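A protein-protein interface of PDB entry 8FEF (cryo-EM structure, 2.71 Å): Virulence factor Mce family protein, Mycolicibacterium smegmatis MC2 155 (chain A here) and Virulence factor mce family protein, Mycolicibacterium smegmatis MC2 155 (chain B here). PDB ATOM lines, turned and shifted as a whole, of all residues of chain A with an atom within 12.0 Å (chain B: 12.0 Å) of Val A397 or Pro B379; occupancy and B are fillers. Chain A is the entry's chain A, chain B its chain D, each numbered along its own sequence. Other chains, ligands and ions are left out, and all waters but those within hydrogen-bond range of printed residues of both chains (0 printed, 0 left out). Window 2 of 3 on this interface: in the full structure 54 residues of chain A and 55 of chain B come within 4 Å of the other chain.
Among the printed residues, merely in contact across the chains: Met A392 with Met B382 (3.2 Å), Ala A394 with Phe B380 (3.3 Å), Tyr A396 with Leu B378 (3.3 Å), Glu A395 with Pro B379 (3.3 Å), Phe A393 with Gly B381 (3.6 Å), Tyr A396 with Tyr B377 (3.6 Å), Pro A391 with Asn B383 (3.8 Å) and Val A397 with Pro B379 (3.8 Å).
The backbone carbonyl oxygen of Phe A393 is in hydrogen-bond range of the backbone NH of Val A402. The backbone NH (N) of Glu A395 lies within hydrogen-bond range of the backbone carbonyl oxygen (O) of Arg A400 (3.1 Å).
N of Tyr A396 lies within hydrogen-bond range of O of Pro B379. The backbone carbonyl oxygen (O) of Met A392 is in hydrogen-bond range of the backbone NH (N) of Asn B383 (2.9 Å). O of Ala A394 sits at hydrogen-bond distance from N of Gly B381 (2.9 Å).
Printed residues of chain A that touch a printed residue of chain B: Pro A391, Met A392, Phe A393, Ala A394, Glu A395, Tyr A396 and Val A397. Hydrophobic or aromatic side chains of chain A within 4 Å of the printed part of chain B: Met A392, Phe A393, Tyr A396 and Val A397. Of the 13 printed residues of chain B, 7 touch a printed residue of chain A. Printed residues of chain B that touch a printed residue of chain A: Tyr B377, Leu B378, Pro B379, Phe B380, Gly B381, Met B382 and Asn B383. Among the printed residues, no Asp or Glu carboxylate lies within 4 Å of a Lys or Arg side-chain nitrogen of the other chain.
Of the printed residues of chain B, Pro A391 touches Asn B383 (3.8 Å). Printed residues of chain B within 4 Å of Phe A393: Gly B381 (3.6 Å). Of chain B, only Pro B379 (3.3 Å) comes within 4 Å of Glu A395. Tyr A396 touches just these residues of chain B: Tyr B377, Leu B378 and Pro B379. No residue of chain B comes within 4 Å of Gly A399. Arg A400 touches none of the printed residues of chain B. Gly B332 touches none of the printed residues of chain A. Of the printed residues of chain A, Tyr B377 touches Tyr A396 (3.6 Å). Leu B378 touches one residue of chain A. Of chain A, only Glu A395 (3.3 Å), Tyr A396 (2.5 Å) and Val A397 (3.8 Å) come within 4 Å of Pro B379. Phe B380 touches just one residue of chain A: Ala A394 (3.3 Å). Gly B381 touches two residues of chain A. Of the printed residues of chain A, Met B382 touches Met A392 (3.2 Å). Of the printed residues of chain A, Asn B383 touches Pro A391 (3.8 Å) and Met A392 (2.9 Å).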
ATOM      1  N   PRO A 391      38.729  10.596  29.932  1.00  0.00           N
ATOM      2  CA  PRO A 391      37.802  11.403  29.112  1.00  0.00           C
ATOM      3  C   PRO A 391      37.943  12.884  29.444  1.00  0.00           C
ATOM      4  O   PRO A 391      37.096  13.497  30.104  1.00  0.00           O
ATOM      5  CB  PRO A 391      36.430  10.831  29.495  1.00  0.00           C
ATOM      6  CG  PRO A 391      36.698   9.602  30.315  1.00  0.00           C
ATOM      7  CD  PRO A 391      37.997   9.862  30.976  1.00  0.00           C
ATOM      8  N   MET A 392      39.058  13.467  28.993  1.00  0.00           N
ATOM      9  CA  MET A 392      39.422  14.825  29.392  1.00  0.00           C
ATOM     10  C   MET A 392      38.375  15.841  28.952  1.00  0.00           C
ATOM     11  O   MET A 392      37.974  16.709  29.731  1.00  0.00           O
ATOM     12  CB  MET A 392      40.790  15.187  28.815  1.00  0.00           C
ATOM     13  CG  MET A 392      41.454  16.374  29.490  1.00  0.00           C
ATOM     14  SD  MET A 392      43.074  16.745  28.795  1.00  0.00           S
ATOM     15  CE  MET A 392      43.834  15.126  28.826  1.00  0.00           C
ATOM     16  N   PHE A 393      37.925  15.751  27.705  1.00  0.00           N
ATOM     17  CA  PHE A 393      36.901  16.636  27.170  1.00  0.00           C
ATOM     18  C   PHE A 393      35.745  15.788  26.666  1.00  0.00           C
ATOM     19  O   PHE A 393      35.963  14.781  25.985  1.00  0.00           O
ATOM     20  CB  PHE A 393      37.466  17.514  26.047  1.00  0.00           C
ATOM     21  CG  PHE A 393      36.418  18.206  25.218  1.00  0.00           C
ATOM     22  CD1 PHE A 393      35.801  19.358  25.678  1.00  0.00           C
ATOM     23  CD2 PHE A 393      36.073  17.723  23.965  1.00  0.00           C
ATOM     24  CE1 PHE A 393      34.845  20.001  24.913  1.00  0.00           C
ATOM     25  CE2 PHE A 393      35.119  18.362  23.198  1.00  0.00           C
ATOM     26  CZ  PHE A 393      34.505  19.501  23.672  1.00  0.00           C
ATOM     27  N   ALA A 394      34.525  16.183  27.013  1.00  0.00           N
ATOM     28  CA  ALA A 394      33.334  15.438  26.642  1.00  0.00           C
ATOM     29  C   ALA A 394      32.273  16.395  26.123  1.00  0.00           C
ATOM     30  O   ALA A 394      32.195  17.551  26.549  1.00  0.00           O
ATOM     31  CB  ALA A 394      32.777  14.636  27.824  1.00  0.00           C
ATOM     32  N   GLU A 395      31.456  15.903  25.197  1.00  0.00           N
ATOM     33  CA  GLU A 395      30.343  16.665  24.652  1.00  0.00           C
ATOM     34  C   GLU A 395      29.069  15.847  24.790  1.00  0.00           C
ATOM     35  O   GLU A 395      29.081  14.627  24.605  1.00  0.00           O
ATOM     36  CB  GLU A 395      30.587  17.036  23.184  1.00  0.00           C
ATOM     37  CG  GLU A 395      29.438  17.787  22.533  1.00  0.00           C
ATOM     38  CD  GLU A 395      29.828  18.433  21.223  1.00  0.00           C
ATOM     39  OE1 GLU A 395      30.975  18.912  21.114  1.00  0.00           O
ATOM     40  OE2 GLU A 395      28.987  18.460  20.301  1.00  0.00           O
ATOM     41  N   TYR A 396      27.970  16.524  25.122  1.00  0.00           N
ATOM     42  CA  TYR A 396      26.692  15.875  25.376  1.00  0.00           C
ATOM     43  C   TYR A 396      25.658  16.215  24.307  1.00  0.00           C
ATOM     44  O   TYR A 396      24.456  16.231  24.577  1.00  0.00           O
ATOM     45  CB  TYR A 396      26.184  16.252  26.765  1.00  0.00           C
ATOM     46  CG  TYR A 396      27.195  15.969  27.849  1.00  0.00           C
ATOM     47  CD1 TYR A 396      27.860  14.752  27.899  1.00  0.00           C
ATOM     48  CD2 TYR A 396      27.506  16.923  28.804  1.00  0.00           C
ATOM     49  CE1 TYR A 396      28.792  14.487  28.878  1.00  0.00           C
ATOM     50  CE2 TYR A 396      28.437  16.669  29.787  1.00  0.00           C
ATOM     51  CZ  TYR A 396      29.077  15.449  29.819  1.00  0.00           C
ATOM     52  OH  TYR A 396      30.007  15.188  30.797  1.00  0.00           O
ATOM     53  N   VAL A 397      26.118  16.491  23.091  1.00  0.00           N
ATOM     54  CA  VAL A 397      25.250  16.696  21.939  1.00  0.00           C
ATOM     55  C   VAL A 397      25.344  15.526  20.966  1.00  0.00           C
ATOM     56  O   VAL A 397      24.333  14.914  20.618  1.00  0.00           O
ATOM     57  CB  VAL A 397      25.576  18.031  21.233  1.00  0.00           C
ATOM     58  CG1 VAL A 397      24.731  18.186  19.982  1.00  0.00           C
ATOM     59  CG2 VAL A 397      25.350  19.195  22.179  1.00  0.00           C
ATOM     60  N   TRP A 398      26.556  15.198  20.521  1.00  0.00           N
ATOM     61  CA  TRP A 398      26.797  14.033  19.682  1.00  0.00           C
ATOM     62  C   TRP A 398      27.570  12.943  20.413  1.00  0.00           C
ATOM     63  O   TRP A 398      28.025  11.987  19.777  1.00  0.00           O
ATOM     64  CB  TRP A 398      27.544  14.438  18.409  1.00  0.00           C
ATOM     65  CG  TRP A 398      26.744  15.306  17.486  1.00  0.00           C
ATOM     66  CD1 TRP A 398      27.009  16.598  17.142  1.00  0.00           C
ATOM     67  CD2 TRP A 398      25.548  14.943  16.785  1.00  0.00           C
ATOM     68  NE1 TRP A 398      26.055  17.064  16.272  1.00  0.00           N
ATOM     69  CE2 TRP A 398      25.146  16.066  16.036  1.00  0.00           C
ATOM     70  CE3 TRP A 398      24.779  13.777  16.717  1.00  0.00           C
ATOM     71  CZ2 TRP A 398      24.009  16.059  15.231  1.00  0.00           C
ATOM     72  CZ3 TRP A 398      23.651  13.772  15.918  1.00  0.00           C
ATOM     73  CH2 TRP A 398      23.276  14.905  15.187  1.00  0.00           C
ATOM     74  N   GLY A 399      27.727  13.066  21.730  1.00  0.00           N
ATOM     75  CA  GLY A 399      28.399  12.049  22.516  1.00  0.00           C
ATOM     76  C   GLY A 399      29.853  11.838  22.171  1.00  0.00           C
ATOM     77  O   GLY A 399      30.389  10.756  22.420  1.00  0.00           O
ATOM     78  N   ARG A 400      30.514  12.847  21.612  1.00  0.00           N
ATOM     79  CA  ARG A 400      31.905  12.730  21.196  1.00  0.00           C
ATOM     80  C   ARG A 400      32.809  13.249  22.306  1.00  0.00           C
ATOM     81  O   ARG A 400      32.665  14.397  22.743  1.00  0.00           O
ATOM     82  CB  ARG A 400      32.142  13.501  19.899  1.00  0.00           C
ATOM     83  CG  ARG A 400      33.460  13.185  19.219  1.00  0.00           C
ATOM     84  CD  ARG A 400      33.239  12.790  17.768  1.00  0.00           C
ATOM     85  NE  ARG A 400      32.494  13.807  17.035  1.00  0.00           N
ATOM     86  CZ  ARG A 400      32.077  13.672  15.784  1.00  0.00           C
ATOM     87  NH1 ARG A 400      32.315  12.571  15.090  1.00  0.00           N
ATOM     88  NH2 ARG A 400      31.401  14.665  15.215  1.00  0.00           N
ATOM     89  N   GLN A 401      33.736  12.409  22.760  1.00  0.00           N
ATOM     90  CA  GLN A 401      34.627  12.765  23.853  1.00  0.00           C
ATOM     91  C   GLN A 401      36.044  12.324  23.524  1.00  0.00           C
ATOM     92  O   GLN A 401      36.254  11.243  22.968  1.00  0.00           O
ATOM     93  CB  GLN A 401      34.164  12.139  25.177  1.00  0.00           C
ATOM     94  CG  GLN A 401      33.756  10.679  25.086  1.00  0.00           C
ATOM     95  CD  GLN A 401      34.855   9.734  25.522  1.00  0.00           C
ATOM     96  OE1 GLN A 401      36.012  10.127  25.652  1.00  0.00           O
ATOM     97  NE2 GLN A 401      34.494   8.480  25.759  1.00  0.00           N
ATOM     98  N   VAL A 402      37.013  13.169  23.873  1.00  0.00           N
ATOM     99  CA  VAL A 402      38.416  12.869  23.617  1.00  0.00           C
ATOM    100  C   VAL A 402      38.936  11.918  24.687  1.00  0.00           C
ATOM    101  O   VAL A 402      38.420  11.856  25.807  1.00  0.00           O
ATOM    102  CB  VAL A 402      39.252  14.164  23.552  1.00  0.00           C
ATOM    103  CG1 VAL A 402      38.523  15.221  22.740  1.00  0.00           C
ATOM    104  CG2 VAL A 402      39.575  14.679  24.941  1.00  0.00           C
ATOM    105  N   VAL B 329      27.823  19.367  40.758  1.00  0.00           N
ATOM    106  CA  VAL B 329      27.067  19.389  39.510  1.00  0.00           C
ATOM    107  C   VAL B 329      26.251  20.680  39.419  1.00  0.00           C
ATOM    108  O   VAL B 329      25.943  21.333  40.424  1.00  0.00           O
ATOM    109  CB  VAL B 329      26.156  18.158  39.388  1.00  0.00           C
ATOM    110  CG1 VAL B 329      26.937  16.900  39.686  1.00  0.00           C
ATOM    111  CG2 VAL B 329      24.958  18.280  40.317  1.00  0.00           C
ATOM    112  N   LEU B 330      25.903  21.053  38.186  1.00  0.00           N
ATOM    113  CA  LEU B 330      25.156  22.282  37.914  1.00  0.00           C
ATOM    114  C   LEU B 330      23.943  21.959  37.044  1.00  0.00           C
ATOM    115  O   LEU B 330      23.976  22.085  35.815  1.00  0.00           O
ATOM    116  CB  LEU B 330      26.094  23.356  37.338  1.00  0.00           C
ATOM    117  CG  LEU B 330      26.944  23.400  36.050  1.00  0.00           C
ATOM    118  CD1 LEU B 330      26.211  23.763  34.762  1.00  0.00           C
ATOM    119  CD2 LEU B 330      28.138  24.325  36.253  1.00  0.00           C
ATOM    120  N   PRO B 331      22.852  21.494  37.658  1.00  0.00           N
ATOM    121  CA  PRO B 331      21.625  21.241  36.892  1.00  0.00           C
ATOM    122  C   PRO B 331      20.901  22.527  36.528  1.00  0.00           C
ATOM    123  O   PRO B 331      21.402  23.625  36.785  1.00  0.00           O
ATOM    124  CB  PRO B 331      20.784  20.379  37.843  1.00  0.00           C
ATOM    125  CG  PRO B 331      21.726  19.929  38.919  1.00  0.00           C
ATOM    126  CD  PRO B 331      22.740  21.009  39.042  1.00  0.00           C
ATOM    127  N   GLY B 332      19.723  22.401  35.927  1.00  0.00           N
ATOM    128  CA  GLY B 332      18.922  23.558  35.575  1.00  0.00           C
ATOM    129  C   GLY B 332      19.467  24.347  34.402  1.00  0.00           C
ATOM    130  O   GLY B 332      18.880  25.346  33.987  1.00  0.00           O
ATOM    131  N   PHE B 375      17.500  24.298  29.498  1.00  0.00           N
ATOM    132  CA  PHE B 375      18.390  23.161  29.297  1.00  0.00           C
ATOM    133  C   PHE B 375      18.713  22.487  30.624  1.00  0.00           C
ATOM    134  O   PHE B 375      18.748  23.140  31.664  1.00  0.00           O
ATOM    135  CB  PHE B 375      19.676  23.605  28.590  1.00  0.00           C
ATOM    136  CG  PHE B 375      20.468  24.637  29.347  1.00  0.00           C
ATOM    137  CD1 PHE B 375      20.220  25.987  29.169  1.00  0.00           C
ATOM    138  CD2 PHE B 375      21.478  24.258  30.216  1.00  0.00           C
ATOM    139  CE1 PHE B 375      20.950  26.937  29.856  1.00  0.00           C
ATOM    140  CE2 PHE B 375      22.210  25.204  30.904  1.00  0.00           C
ATOM    141  CZ  PHE B 375      21.946  26.544  30.723  1.00  0.00           C
ATOM    142  N   ASN B 376      18.939  21.173  30.586  1.00  0.00           N
ATOM    143  CA  ASN B 376      19.239  20.441  31.811  1.00  0.00           C
ATOM    144  C   ASN B 376      20.622  20.795  32.345  1.00  0.00           C
ATOM    145  O   ASN B 376      20.785  21.067  33.539  1.00  0.00           O
ATOM    146  CB  ASN B 376      19.124  18.936  31.571  1.00  0.00           C
ATOM    147  CG  ASN B 376      17.703  18.498  31.300  1.00  0.00           C
ATOM    148  OD1 ASN B 376      16.755  19.231  31.571  1.00  0.00           O
ATOM    149  ND2 ASN B 376      17.548  17.293  30.768  1.00  0.00           N
ATOM    150  N   TYR B 377      21.627  20.803  31.475  1.00  0.00           N
ATOM    151  CA  TYR B 377      22.990  21.122  31.881  1.00  0.00           C
ATOM    152  C   TYR B 377      23.779  21.558  30.652  1.00  0.00           C
ATOM    153  O   TYR B 377      23.238  21.683  29.551  1.00  0.00           O
ATOM    154  CB  TYR B 377      23.648  19.932  32.588  1.00  0.00           C
ATOM    155  CG  TYR B 377      23.480  18.612  31.875  1.00  0.00           C
ATOM    156  CD1 TYR B 377      24.315  18.255  30.828  1.00  0.00           C
ATOM    157  CD2 TYR B 377      22.493  17.717  32.258  1.00  0.00           C
ATOM    158  CE1 TYR B 377      24.165  17.050  30.174  1.00  0.00           C
ATOM    159  CE2 TYR B 377      22.338  16.509  31.611  1.00  0.00           C
ATOM    160  CZ  TYR B 377      23.178  16.180  30.571  1.00  0.00           C
ATOM    161  OH  TYR B 377      23.031  14.978  29.921  1.00  0.00           O
ATOM    162  N   LEU B 378      25.072  21.794  30.856  1.00  0.00           N
ATOM    163  CA  LEU B 378      25.918  22.305  29.790  1.00  0.00           C
ATOM    164  C   LEU B 378      26.236  21.205  28.780  1.00  0.00           C
ATOM    165  O   LEU B 378      26.424  20.047  29.163  1.00  0.00           O
ATOM    166  CB  LEU B 378      27.213  22.878  30.363  1.00  0.00           C
ATOM    167  CG  LEU B 378      27.076  24.175  31.156  1.00  0.00           C
ATOM    168  CD1 LEU B 378      28.429  24.618  31.685  1.00  0.00           C
ATOM    169  CD2 LEU B 378      26.453  25.258  30.295  1.00  0.00           C
ATOM    170  N   PRO B 379      26.302  21.536  27.488  1.00  0.00           N
ATOM    171  CA  PRO B 379      26.602  20.510  26.474  1.00  0.00           C
ATOM    172  C   PRO B 379      27.984  19.902  26.606  1.00  0.00           C
ATOM    173  O   PRO B 379      28.199  18.787  26.118  1.00  0.00           O
ATOM    174  CB  PRO B 379      26.460  21.271  25.148  1.00  0.00           C
ATOM    175  CG  PRO B 379      25.677  22.491  25.475  1.00  0.00           C
ATOM    176  CD  PRO B 379      26.033  22.848  26.879  1.00  0.00           C
ATOM    177  N   PHE B 380      28.923  20.590  27.246  1.00  0.00           N
ATOM    178  CA  PHE B 380      30.309  20.157  27.310  1.00  0.00           C
ATOM    179  C   PHE B 380      30.727  19.921  28.754  1.00  0.00           C
ATOM    180  O   PHE B 380      30.158  20.494  29.687  1.00  0.00           O
ATOM    181  CB  PHE B 380      31.239  21.188  26.662  1.00  0.00           C
ATOM    182  CG  PHE B 380      30.884  22.612  26.981  1.00  0.00           C
ATOM    183  CD1 PHE B 380      31.214  23.167  28.207  1.00  0.00           C
ATOM    184  CD2 PHE B 380      30.227  23.400  26.051  1.00  0.00           C
ATOM    185  CE1 PHE B 380      30.890  24.475  28.500  1.00  0.00           C
ATOM    186  CE2 PHE B 380      29.902  24.709  26.338  1.00  0.00           C
ATOM    187  CZ  PHE B 380      30.234  25.247  27.565  1.00  0.00           C
ATOM    188  N   GLY B 381      31.731  19.068  28.925  1.00  0.00           N
ATOM    189  CA  GLY B 381      32.264  18.774  30.241  1.00  0.00           C
ATOM    190  C   GLY B 381      33.752  18.520  30.155  1.00  0.00           C
ATOM    191  O   GLY B 381      34.293  18.241  29.082  1.00  0.00           O
ATOM    192  N   MET B 382      34.414  18.620  31.305  1.00  0.00           N
ATOM    193  CA  MET B 382      35.859  18.478  31.360  1.00  0.00           C
ATOM    194  C   MET B 382      36.267  17.763  32.637  1.00  0.00           C
ATOM    195  O   MET B 382      35.668  17.973  33.696  1.00  0.00           O
ATOM    196  CB  MET B 382      36.553  19.842  31.278  1.00  0.00           C
ATOM    197  CG  MET B 382      37.975  19.784  30.747  1.00  0.00           C
ATOM    198  SD  MET B 382      38.572  21.398  30.210  1.00  0.00           S
ATOM    199  CE  MET B 382      39.909  20.917  29.119  1.00  0.00           C
ATOM    200  N   ASN B 383      37.290  16.918  32.527  1.00  0.00           N
ATOM    201  CA  ASN B 383      37.878  16.202  33.659  1.00  0.00           C
ATOM    202  C   ASN B 383      39.390  16.351  33.518  1.00  0.00           C
ATOM    203  O   ASN B 383      40.039  15.524  32.871  1.00  0.00           O
ATOM    204  CB  ASN B 383      37.445  14.741  33.665  1.00  0.00           C
ATOM    205  CG  ASN B 383      37.889  14.004  34.904  1.00  0.00           C
ATOM    206  OD1 ASN B 383      38.987  13.453  34.958  1.00  0.00           O
ATOM    207  ND2 ASN B 383      37.027  13.974  35.907  1.00  0.00           N
